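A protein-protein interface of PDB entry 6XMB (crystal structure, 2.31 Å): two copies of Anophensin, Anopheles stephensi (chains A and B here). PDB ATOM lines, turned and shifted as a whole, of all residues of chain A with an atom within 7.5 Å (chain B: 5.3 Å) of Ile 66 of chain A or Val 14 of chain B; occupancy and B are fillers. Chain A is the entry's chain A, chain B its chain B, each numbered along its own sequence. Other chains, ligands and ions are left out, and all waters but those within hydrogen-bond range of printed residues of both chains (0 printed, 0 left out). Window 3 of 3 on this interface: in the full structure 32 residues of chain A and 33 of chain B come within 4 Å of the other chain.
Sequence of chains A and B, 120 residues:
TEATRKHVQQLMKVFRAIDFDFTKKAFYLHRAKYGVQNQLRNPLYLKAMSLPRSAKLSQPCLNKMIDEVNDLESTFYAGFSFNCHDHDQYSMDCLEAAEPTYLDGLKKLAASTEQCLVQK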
ATOM      1  N   LEU A  40      15.513  -7.410  15.697  1.00  0.00           N
ATOM      2  CA  LEU A  40      15.171  -7.333  14.287  1.00  0.00           C
ATOM      3  C   LEU A  40      16.409  -7.378  13.411  1.00  0.00           C
ATOM      4  O   LEU A  40      16.542  -8.272  12.573  1.00  0.00           O
ATOM      5  CB  LEU A  40      14.364  -6.063  14.010  1.00  0.00           C
ATOM      6  CG  LEU A  40      13.869  -5.889  12.577  1.00  0.00           C
ATOM      7  CD1 LEU A  40      12.916  -7.003  12.229  1.00  0.00           C
ATOM      8  CD2 LEU A  40      13.177  -4.546  12.392  1.00  0.00           C
ATOM      9  N   TYR A  45      20.223 -10.358  10.068  1.00  0.00           N
ATOM     10  CA  TYR A  45      21.582 -10.509   9.565  1.00  0.00           C
ATOM     11  C   TYR A  45      21.974 -11.974   9.487  1.00  0.00           C
ATOM     12  O   TYR A  45      22.758 -12.354   8.612  1.00  0.00           O
ATOM     13  CB  TYR A  45      22.582  -9.759  10.444  1.00  0.00           C
ATOM     14  CG  TYR A  45      22.732  -8.288  10.111  1.00  0.00           C
ATOM     15  CD1 TYR A  45      22.271  -7.774   8.902  1.00  0.00           C
ATOM     16  CD2 TYR A  45      23.350  -7.410  11.002  1.00  0.00           C
ATOM     17  CE1 TYR A  45      22.413  -6.414   8.592  1.00  0.00           C
ATOM     18  CE2 TYR A  45      23.500  -6.062  10.697  1.00  0.00           C
ATOM     19  CZ  TYR A  45      23.031  -5.574   9.497  1.00  0.00           C
ATOM     20  OH  TYR A  45      23.178  -4.243   9.204  1.00  0.00           O
ATOM     21  N   GLN A  59      12.234  -6.527  -2.277  1.00  0.00           N
ATOM     22  CA  GLN A  59      12.222  -5.193  -1.687  1.00  0.00           C
ATOM     23  C   GLN A  59      10.835  -4.762  -1.206  1.00  0.00           C
ATOM     24  O   GLN A  59      10.754  -3.954  -0.273  1.00  0.00           O
ATOM     25  CB  GLN A  59      12.787  -4.152  -2.651  1.00  0.00           C
ATOM     26  CG  GLN A  59      13.400  -2.968  -1.906  1.00  0.00           C
ATOM     27  CD  GLN A  59      12.922  -1.642  -2.450  1.00  0.00           C
ATOM     28  OE1 GLN A  59      12.670  -1.505  -3.646  1.00  0.00           O
ATOM     29  NE2 GLN A  59      12.788  -0.654  -1.569  1.00  0.00           N
ATOM     30  N   PRO A  60       9.726  -5.235  -1.793  1.00  0.00           N
ATOM     31  CA  PRO A  60       8.434  -5.059  -1.103  1.00  0.00           C
ATOM     32  C   PRO A  60       8.462  -5.538   0.337  1.00  0.00           C
ATOM     33  O   PRO A  60       7.754  -4.989   1.187  1.00  0.00           O
ATOM     34  CB  PRO A  60       7.470  -5.903  -1.946  1.00  0.00           C
ATOM     35  CG  PRO A  60       8.039  -5.851  -3.305  1.00  0.00           C
ATOM     36  CD  PRO A  60       9.535  -5.778  -3.153  1.00  0.00           C
ATOM     37  N   CYS A  61       9.268  -6.561   0.632  1.00  0.00           N
ATOM     38  CA  CYS A  61       9.358  -7.097   1.984  1.00  0.00           C
ATOM     39  C   CYS A  61      10.158  -6.166   2.887  1.00  0.00           C
ATOM     40  O   CYS A  61       9.787  -5.948   4.046  1.00  0.00           O
ATOM     41  CB  CYS A  61       9.984  -8.497   1.939  1.00  0.00           C
ATOM     42  SG  CYS A  61      10.216  -9.367   3.525  1.00  0.00           S
ATOM     43  N   LEU A  62      11.257  -5.607   2.374  1.00  0.00           N
ATOM     44  CA  LEU A  62      11.997  -4.607   3.137  1.00  0.00           C
ATOM     45  C   LEU A  62      11.152  -3.364   3.356  1.00  0.00           C
ATOM     46  O   LEU A  62      11.216  -2.737   4.421  1.00  0.00           O
ATOM     47  CB  LEU A  62      13.296  -4.245   2.417  1.00  0.00           C
ATOM     48  CG  LEU A  62      14.301  -5.377   2.208  1.00  0.00           C
ATOM     49  CD1 LEU A  62      15.447  -4.906   1.329  1.00  0.00           C
ATOM     50  CD2 LEU A  62      14.827  -5.901   3.544  1.00  0.00           C
ATOM     51  N   ASN A  63      10.341  -3.001   2.360  1.00  0.00           N
ATOM     52  CA  ASN A  63       9.466  -1.842   2.491  1.00  0.00           C
ATOM     53  C   ASN A  63       8.416  -2.059   3.574  1.00  0.00           C
ATOM     54  O   ASN A  63       8.204  -1.185   4.421  1.00  0.00           O
ATOM     55  CB  ASN A  63       8.810  -1.528   1.146  1.00  0.00           C
ATOM     56  CG  ASN A  63       9.792  -0.956   0.146  1.00  0.00           C
ATOM     57  OD1 ASN A  63      10.800  -0.341   0.527  1.00  0.00           O
ATOM     58  ND2 ASN A  63       9.515  -1.159  -1.140  1.00  0.00           N
ATOM     59  N   LYS A  64       7.754  -3.222   3.574  1.00  0.00           N
ATOM     60  CA  LYS A  64       6.818  -3.534   4.650  1.00  0.00           C
ATOM     61  C   LYS A  64       7.498  -3.463   6.016  1.00  0.00           C
ATOM     62  O   LYS A  64       6.922  -2.923   6.971  1.00  0.00           O
ATOM     63  CB  LYS A  64       6.199  -4.916   4.439  1.00  0.00           C
ATOM     64  CG  LYS A  64       5.282  -5.346   5.582  1.00  0.00           C
ATOM     65  CD  LYS A  64       4.091  -6.163   5.105  1.00  0.00           C
ATOM     66  CE  LYS A  64       4.442  -7.623   4.923  1.00  0.00           C
ATOM     67  NZ  LYS A  64       4.593  -8.284   6.243  1.00  0.00           N
ATOM     68  N   MET A  65       8.728  -3.990   6.125  1.00  0.00           N
ATOM     69  CA  MET A  65       9.463  -3.970   7.394  1.00  0.00           C
ATOM     70  C   MET A  65       9.711  -2.545   7.879  1.00  0.00           C
ATOM     71  O   MET A  65       9.433  -2.216   9.039  1.00  0.00           O
ATOM     72  CB  MET A  65      10.790  -4.718   7.244  1.00  0.00           C
ATOM     73  CG  MET A  65      11.560  -4.896   8.543  1.00  0.00           C
ATOM     74  SD  MET A  65      13.313  -5.294   8.297  1.00  0.00           S
ATOM     75  CE  MET A  65      13.919  -3.736   7.693  1.00  0.00           C
ATOM     76  N   ILE A  66      10.241  -1.685   7.007  1.00  0.00           N
ATOM     77  CA  ILE A  66      10.504  -0.297   7.391  1.00  0.00           C
ATOM     78  C   ILE A  66       9.239   0.363   7.918  1.00  0.00           C
ATOM     79  O   ILE A  66       9.228   0.948   9.001  1.00  0.00           O
ATOM     80  CB  ILE A  66      11.068   0.500   6.204  1.00  0.00           C
ATOM     81  CG1 ILE A  66      12.470   0.035   5.830  1.00  0.00           C
ATOM     82  CG2 ILE A  66      11.048   1.991   6.528  1.00  0.00           C
ATOM     83  CD1 ILE A  66      12.884   0.488   4.437  1.00  0.00           C
ATOM     84  N   ASP A  67       8.149   0.297   7.155  1.00  0.00           N
ATOM     85  CA  ASP A  67       6.950   0.976   7.626  1.00  0.00           C
ATOM     86  C   ASP A  67       6.397   0.309   8.878  1.00  0.00           C
ATOM     87  O   ASP A  67       5.813   0.986   9.730  1.00  0.00           O
ATOM     88  CB  ASP A  67       5.912   1.028   6.511  1.00  0.00           C
ATOM     89  CG  ASP A  67       6.286   2.021   5.434  1.00  0.00           C
ATOM     90  OD1 ASP A  67       6.521   3.209   5.785  1.00  0.00           O
ATOM     91  OD2 ASP A  67       6.376   1.602   4.252  1.00  0.00           O
ATOM     92  N   GLU A  68       6.589  -1.004   9.015  1.00  0.00           N
ATOM     93  CA  GLU A  68       6.207  -1.679  10.249  1.00  0.00           C
ATOM     94  C   GLU A  68       7.153  -1.331  11.399  1.00  0.00           C
ATOM     95  O   GLU A  68       6.731  -1.313  12.560  1.00  0.00           O
ATOM     96  CB  GLU A  68       6.164  -3.193  10.036  1.00  0.00           C
ATOM     97  N   VAL A  69       8.423  -1.038  11.119  1.00  0.00           N
ATOM     98  CA  VAL A  69       9.258  -0.506  12.196  1.00  0.00           C
ATOM     99  C   VAL A  69       8.686   0.806  12.702  1.00  0.00           C
ATOM    100  O   VAL A  69       8.595   1.033  13.916  1.00  0.00           O
ATOM    101  CB  VAL A  69      10.715  -0.345  11.737  1.00  0.00           C
ATOM    102  CG1 VAL A  69      11.455   0.594  12.665  1.00  0.00           C
ATOM    103  CG2 VAL A  69      11.397  -1.694  11.715  1.00  0.00           C
ATOM    104  N   ASN A  70       8.250   1.672  11.779  1.00  0.00           N
ATOM    105  CA  ASN A  70       7.767   3.006  12.145  1.00  0.00           C
ATOM    106  C   ASN A  70       6.512   2.940  12.998  1.00  0.00           C
ATOM    107  O   ASN A  70       6.354   3.709  13.950  1.00  0.00           O
ATOM    108  CB  ASN A  70       7.485   3.825  10.887  1.00  0.00           C
ATOM    109  CG  ASN A  70       8.736   4.378  10.270  1.00  0.00           C
ATOM    110  OD1 ASN A  70       9.618   4.874  10.980  1.00  0.00           O
ATOM    111  ND2 ASN A  70       8.838   4.291   8.947  1.00  0.00           N
ATOM    112  N   ASP A  71       5.593   2.051  12.653  1.00  0.00           N
ATOM    113  CA  ASP A  71       4.346   1.985  13.397  1.00  0.00           C
ATOM    114  C   ASP A  71       4.559   1.406  14.789  1.00  0.00           C
ATOM    115  O   ASP A  71       3.944   1.865  15.755  1.00  0.00           O
ATOM    116  CB  ASP A  71       3.324   1.183  12.597  1.00  0.00           C
ATOM    117  CG  ASP A  71       2.601   2.044  11.581  1.00  0.00           C
ATOM    118  OD1 ASP A  71       1.807   2.911  12.012  1.00  0.00           O
ATOM    119  OD2 ASP A  71       2.839   1.896  10.354  1.00  0.00           O
ATOM    120  N   LEU A  72       5.416   0.389  14.911  1.00  0.00           N
ATOM    121  CA  LEU A  72       5.724  -0.155  16.229  1.00  0.00           C
ATOM    122  C   LEU A  72       6.380   0.898  17.115  1.00  0.00           C
ATOM    123  O   LEU A  72       6.047   1.018  18.298  1.00  0.00           O
ATOM    124  CB  LEU A  72       6.626  -1.385  16.099  1.00  0.00           C
ATOM    125  CG  LEU A  72       6.038  -2.587  15.329  1.00  0.00           C
ATOM    126  CD1 LEU A  72       7.125  -3.611  15.065  1.00  0.00           C
ATOM    127  CD2 LEU A  72       4.888  -3.213  16.079  1.00  0.00           C
ATOM    128  N   LEU A 109       7.869  -9.283  13.873  1.00  0.00           N
ATOM    129  CA  LEU A 109       8.187  -8.707  12.569  1.00  0.00           C
ATOM    130  C   LEU A 109       9.428  -9.354  11.971  1.00  0.00           C
ATOM    131  O   LEU A 109       9.505  -9.563  10.755  1.00  0.00           O
ATOM    132  CB  LEU A 109       8.378  -7.194  12.677  1.00  0.00           C
ATOM    133  CG  LEU A 109       8.952  -6.521  11.423  1.00  0.00           C
ATOM    134  CD1 LEU A 109       8.033  -6.747  10.224  1.00  0.00           C
ATOM    135  CD2 LEU A 109       9.124  -5.046  11.672  1.00  0.00           C
ATOM    136  N   THR A 113       9.337 -11.038   8.278  1.00  0.00           N
ATOM    137  CA  THR A 113      10.319 -10.513   7.335  1.00  0.00           C
ATOM    138  C   THR A 113      11.230 -11.621   6.829  1.00  0.00           C
ATOM    139  O   THR A 113      11.582 -11.654   5.645  1.00  0.00           O
ATOM    140  CB  THR A 113      11.149  -9.405   7.990  1.00  0.00           C
ATOM    141  OG1 THR A 113      10.273  -8.433   8.560  1.00  0.00           O
ATOM    142  CG2 THR A 113      12.033  -8.731   6.972  1.00  0.00           C
ATOM    143  N   GLN B  10      23.292  -5.151   1.480  1.00  0.00           N
ATOM    144  CA  GLN B  10      21.968  -4.647   1.132  1.00  0.00           C
ATOM    145  C   GLN B  10      21.086  -4.492   2.365  1.00  0.00           C
ATOM    146  O   GLN B  10      20.300  -3.540   2.445  1.00  0.00           O
ATOM    147  CB  GLN B  10      21.307  -5.572   0.110  1.00  0.00           C
ATOM    148  CG  GLN B  10      19.960  -5.101  -0.429  1.00  0.00           C
ATOM    149  CD  GLN B  10      19.412  -6.035  -1.520  1.00  0.00           C
ATOM    150  OE1 GLN B  10      20.176  -6.652  -2.272  1.00  0.00           O
ATOM    151  NE2 GLN B  10      18.089  -6.146  -1.598  1.00  0.00           N
ATOM    152  N   LEU B  11      21.201  -5.402   3.334  1.00  0.00           N
ATOM    153  CA  LEU B  11      20.440  -5.252   4.571  1.00  0.00           C
ATOM    154  C   LEU B  11      20.999  -4.139   5.446  1.00  0.00           C
ATOM    155  O   LEU B  11      20.241  -3.482   6.166  1.00  0.00           O
ATOM    156  CB  LEU B  11      20.420  -6.561   5.359  1.00  0.00           C
ATOM    157  CG  LEU B  11      19.299  -7.542   5.042  1.00  0.00           C
ATOM    158  CD1 LEU B  11      19.286  -8.677   6.046  1.00  0.00           C
ATOM    159  CD2 LEU B  11      17.974  -6.809   5.047  1.00  0.00           C
ATOM    160  N   MET B  12      22.315  -3.925   5.422  1.00  0.00           N
ATOM    161  CA  MET B  12      22.885  -2.871   6.249  1.00  0.00           C
ATOM    162  C   MET B  12      22.374  -1.510   5.809  1.00  0.00           C
ATOM    163  O   MET B  12      22.114  -0.637   6.644  1.00  0.00           O
ATOM    164  CB  MET B  12      24.411  -2.920   6.206  1.00  0.00           C
ATOM    165  CG  MET B  12      25.083  -1.838   7.066  1.00  0.00           C
ATOM    166  SD  MET B  12      26.663  -2.378   7.753  1.00  0.00           S
ATOM    167  CE  MET B  12      27.128  -3.618   6.528  1.00  0.00           C
ATOM    168  N   LYS B  13      22.196  -1.327   4.496  1.00  0.00           N
ATOM    169  CA  LYS B  13      21.681  -0.066   3.974  1.00  0.00           C
ATOM    170  C   LYS B  13      20.365   0.305   4.648  1.00  0.00           C
ATOM    171  O   LYS B  13      20.191   1.433   5.128  1.00  0.00           O
ATOM    172  CB  LYS B  13      21.512  -0.166   2.459  1.00  0.00           C
ATOM    173  CG  LYS B  13      21.264   1.160   1.785  1.00  0.00           C
ATOM    174  CD  LYS B  13      21.677   1.118   0.318  1.00  0.00           C
ATOM    175  CE  LYS B  13      21.191   2.358  -0.408  1.00  0.00           C
ATOM    176  NZ  LYS B  13      19.723   2.506  -0.205  1.00  0.00           N
ATOM    177  N   VAL B  14      19.444  -0.655   4.737  1.00  0.00           N
ATOM    178  CA  VAL B  14      18.154  -0.406   5.372  1.00  0.00           C
ATOM    179  C   VAL B  14      18.315  -0.128   6.861  1.00  0.00           C
ATOM    180  O   VAL B  14      17.626   0.731   7.421  1.00  0.00           O
ATOM    181  CB  VAL B  14      17.214  -1.596   5.126  1.00  0.00           C
ATOM    182  CG1 VAL B  14      16.013  -1.508   6.043  1.00  0.00           C
ATOM    183  CG2 VAL B  14      16.803  -1.651   3.656  1.00  0.00           C
ATOM    184  N   PHE B  15      19.184  -0.871   7.541  1.00  0.00           N
ATOM    185  CA  PHE B  15      19.317  -0.664   8.978  1.00  0.00           C
ATOM    186  C   PHE B  15      20.188   0.532   9.308  1.00  0.00           C
ATOM    187  O   PHE B  15      20.031   1.110  10.382  1.00  0.00           O
ATOM    188  CB  PHE B  15      19.849  -1.933   9.656  1.00  0.00           C
ATOM    189  CG  PHE B  15      18.809  -2.991   9.787  1.00  0.00           C
ATOM    190  CD1 PHE B  15      17.821  -2.879  10.749  1.00  0.00           C
ATOM    191  CD2 PHE B  15      18.772  -4.059   8.912  1.00  0.00           C
ATOM    192  CE1 PHE B  15      16.832  -3.815  10.856  1.00  0.00           C
ATOM    193  CE2 PHE B  15      17.786  -5.011   9.014  1.00  0.00           C
ATOM    194  CZ  PHE B  15      16.810  -4.893   9.976  1.00  0.00           C
ATOM    195  N   ARG B  16      21.096   0.905   8.407  1.00  0.00           N
ATOM    196  CA  ARG B  16      21.790   2.178   8.543  1.00  0.00           C
ATOM    197  C   ARG B  16      20.796   3.332   8.590  1.00  0.00           C
ATOM    198  O   ARG B  16      20.891   4.198   9.465  1.00  0.00           O
ATOM    199  CB  ARG B  16      22.780   2.367   7.391  1.00  0.00           C
ATOM    200  CG  ARG B  16      23.752   3.514   7.614  1.00  0.00           C
ATOM    201  CD  ARG B  16      24.558   3.829   6.377  1.00  0.00           C
ATOM    202  NE  ARG B  16      25.430   2.729   5.988  1.00  0.00           N
ATOM    203  CZ  ARG B  16      25.244   1.963   4.916  1.00  0.00           C
ATOM    204  NH1 ARG B  16      24.215   2.185   4.116  1.00  0.00           N
ATOM    205  NH2 ARG B  16      26.097   0.984   4.640  1.00  0.00           N
ATOM    206  N   ALA B  17      19.808   3.334   7.687  1.00  0.00           N
ATOM    207  CA  ALA B  17      18.846   4.433   7.637  1.00  0.00           C
ATOM    208  C   ALA B  17      18.004   4.497   8.899  1.00  0.00           C
ATOM    209  O   ALA B  17      17.736   5.592   9.414  1.00  0.00           O
ATOM    210  CB  ALA B  17      17.936   4.304   6.419  1.00  0.00           C
ATOM    211  N   ILE B  18      17.574   3.349   9.417  1.00  0.00           N
ATOM    212  CA  ILE B  18      16.799   3.370  10.651  1.00  0.00           C
ATOM    213  C   ILE B  18      17.645   3.925  11.792  1.00  0.00           C
ATOM    214  O   ILE B  18      17.165   4.695  12.632  1.00  0.00           O
ATOM    215  CB  ILE B  18      16.264   1.966  10.955  1.00  0.00           C
ATOM    216  CG1 ILE B  18      15.149   1.606   9.965  1.00  0.00           C
ATOM    217  CG2 ILE B  18      15.782   1.875  12.372  1.00  0.00           C
ATOM    218  CD1 ILE B  18      14.689   0.153  10.099  1.00  0.00           C
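No position is printed for both chains.
Of the printed residues of chain B, Tyr 45 of chain A touches Leu 11 (3.8 Å) and Met 12 (3.3 Å).
Gln 59 of chain A touches none of the printed residues of chain B.
Printed residues of chain B within 4 Å of Leu 62 of chain A: Leu 11.
Of the printed residues of chain B, Met 65 of chain A touches Val 14 (3.5 Å) and Phe 15 (3.9 Å).
Of the printed residues of chain B, Ile 66 of chain A touches Val 14.
Leu 109 of chain A touches none of the printed residues of chain B.
Printed residues of chain A within 4 Å of Leu 11 of chain B: Tyr 45 and Leu 62.
Of the printed residues of chain A, Phe 15 of chain B touches Met 65 (3.9 Å).
The nearest residue of chain B that does not touch Ile 66 of chain A is Ile 18 of chain B (4.8 Å).
The nearest residue of chain A that does not touch Val 14 of chain B is Leu 62 of chain A (4.2 Å).
Among the printed residues, merely in contact across the chains: Tyr 45 of chain A with Met 12 of chain B (3.3 Å), Met 65 of chain A with Val 14 of chain B (3.5 Å), Leu 62 of chain A with Leu 11 of chain B (3.6 Å), Tyr 45 of chain A with Leu 11 of chain B (3.8 Å), Met 65 of chain A with Phe 15 of chain B (3.9 Å) and Ile 66 of chain A with Val 14 of chain B (3.9 Å).
Of the 18 printed residues of chain A, 4 touch a printed residue of chain B.
Of the 9 printed residues of chain B, 4 touch a printed residue of chain A.
Among the printed residues, 6 pairs touch across the chains.
The backbone carbonyl oxygen (O) of Ile 66 of chain A sits at hydrogen-bond distance from the side-chain amide nitrogen (ND2) of Asn 70 of chain A (3.4 Å).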
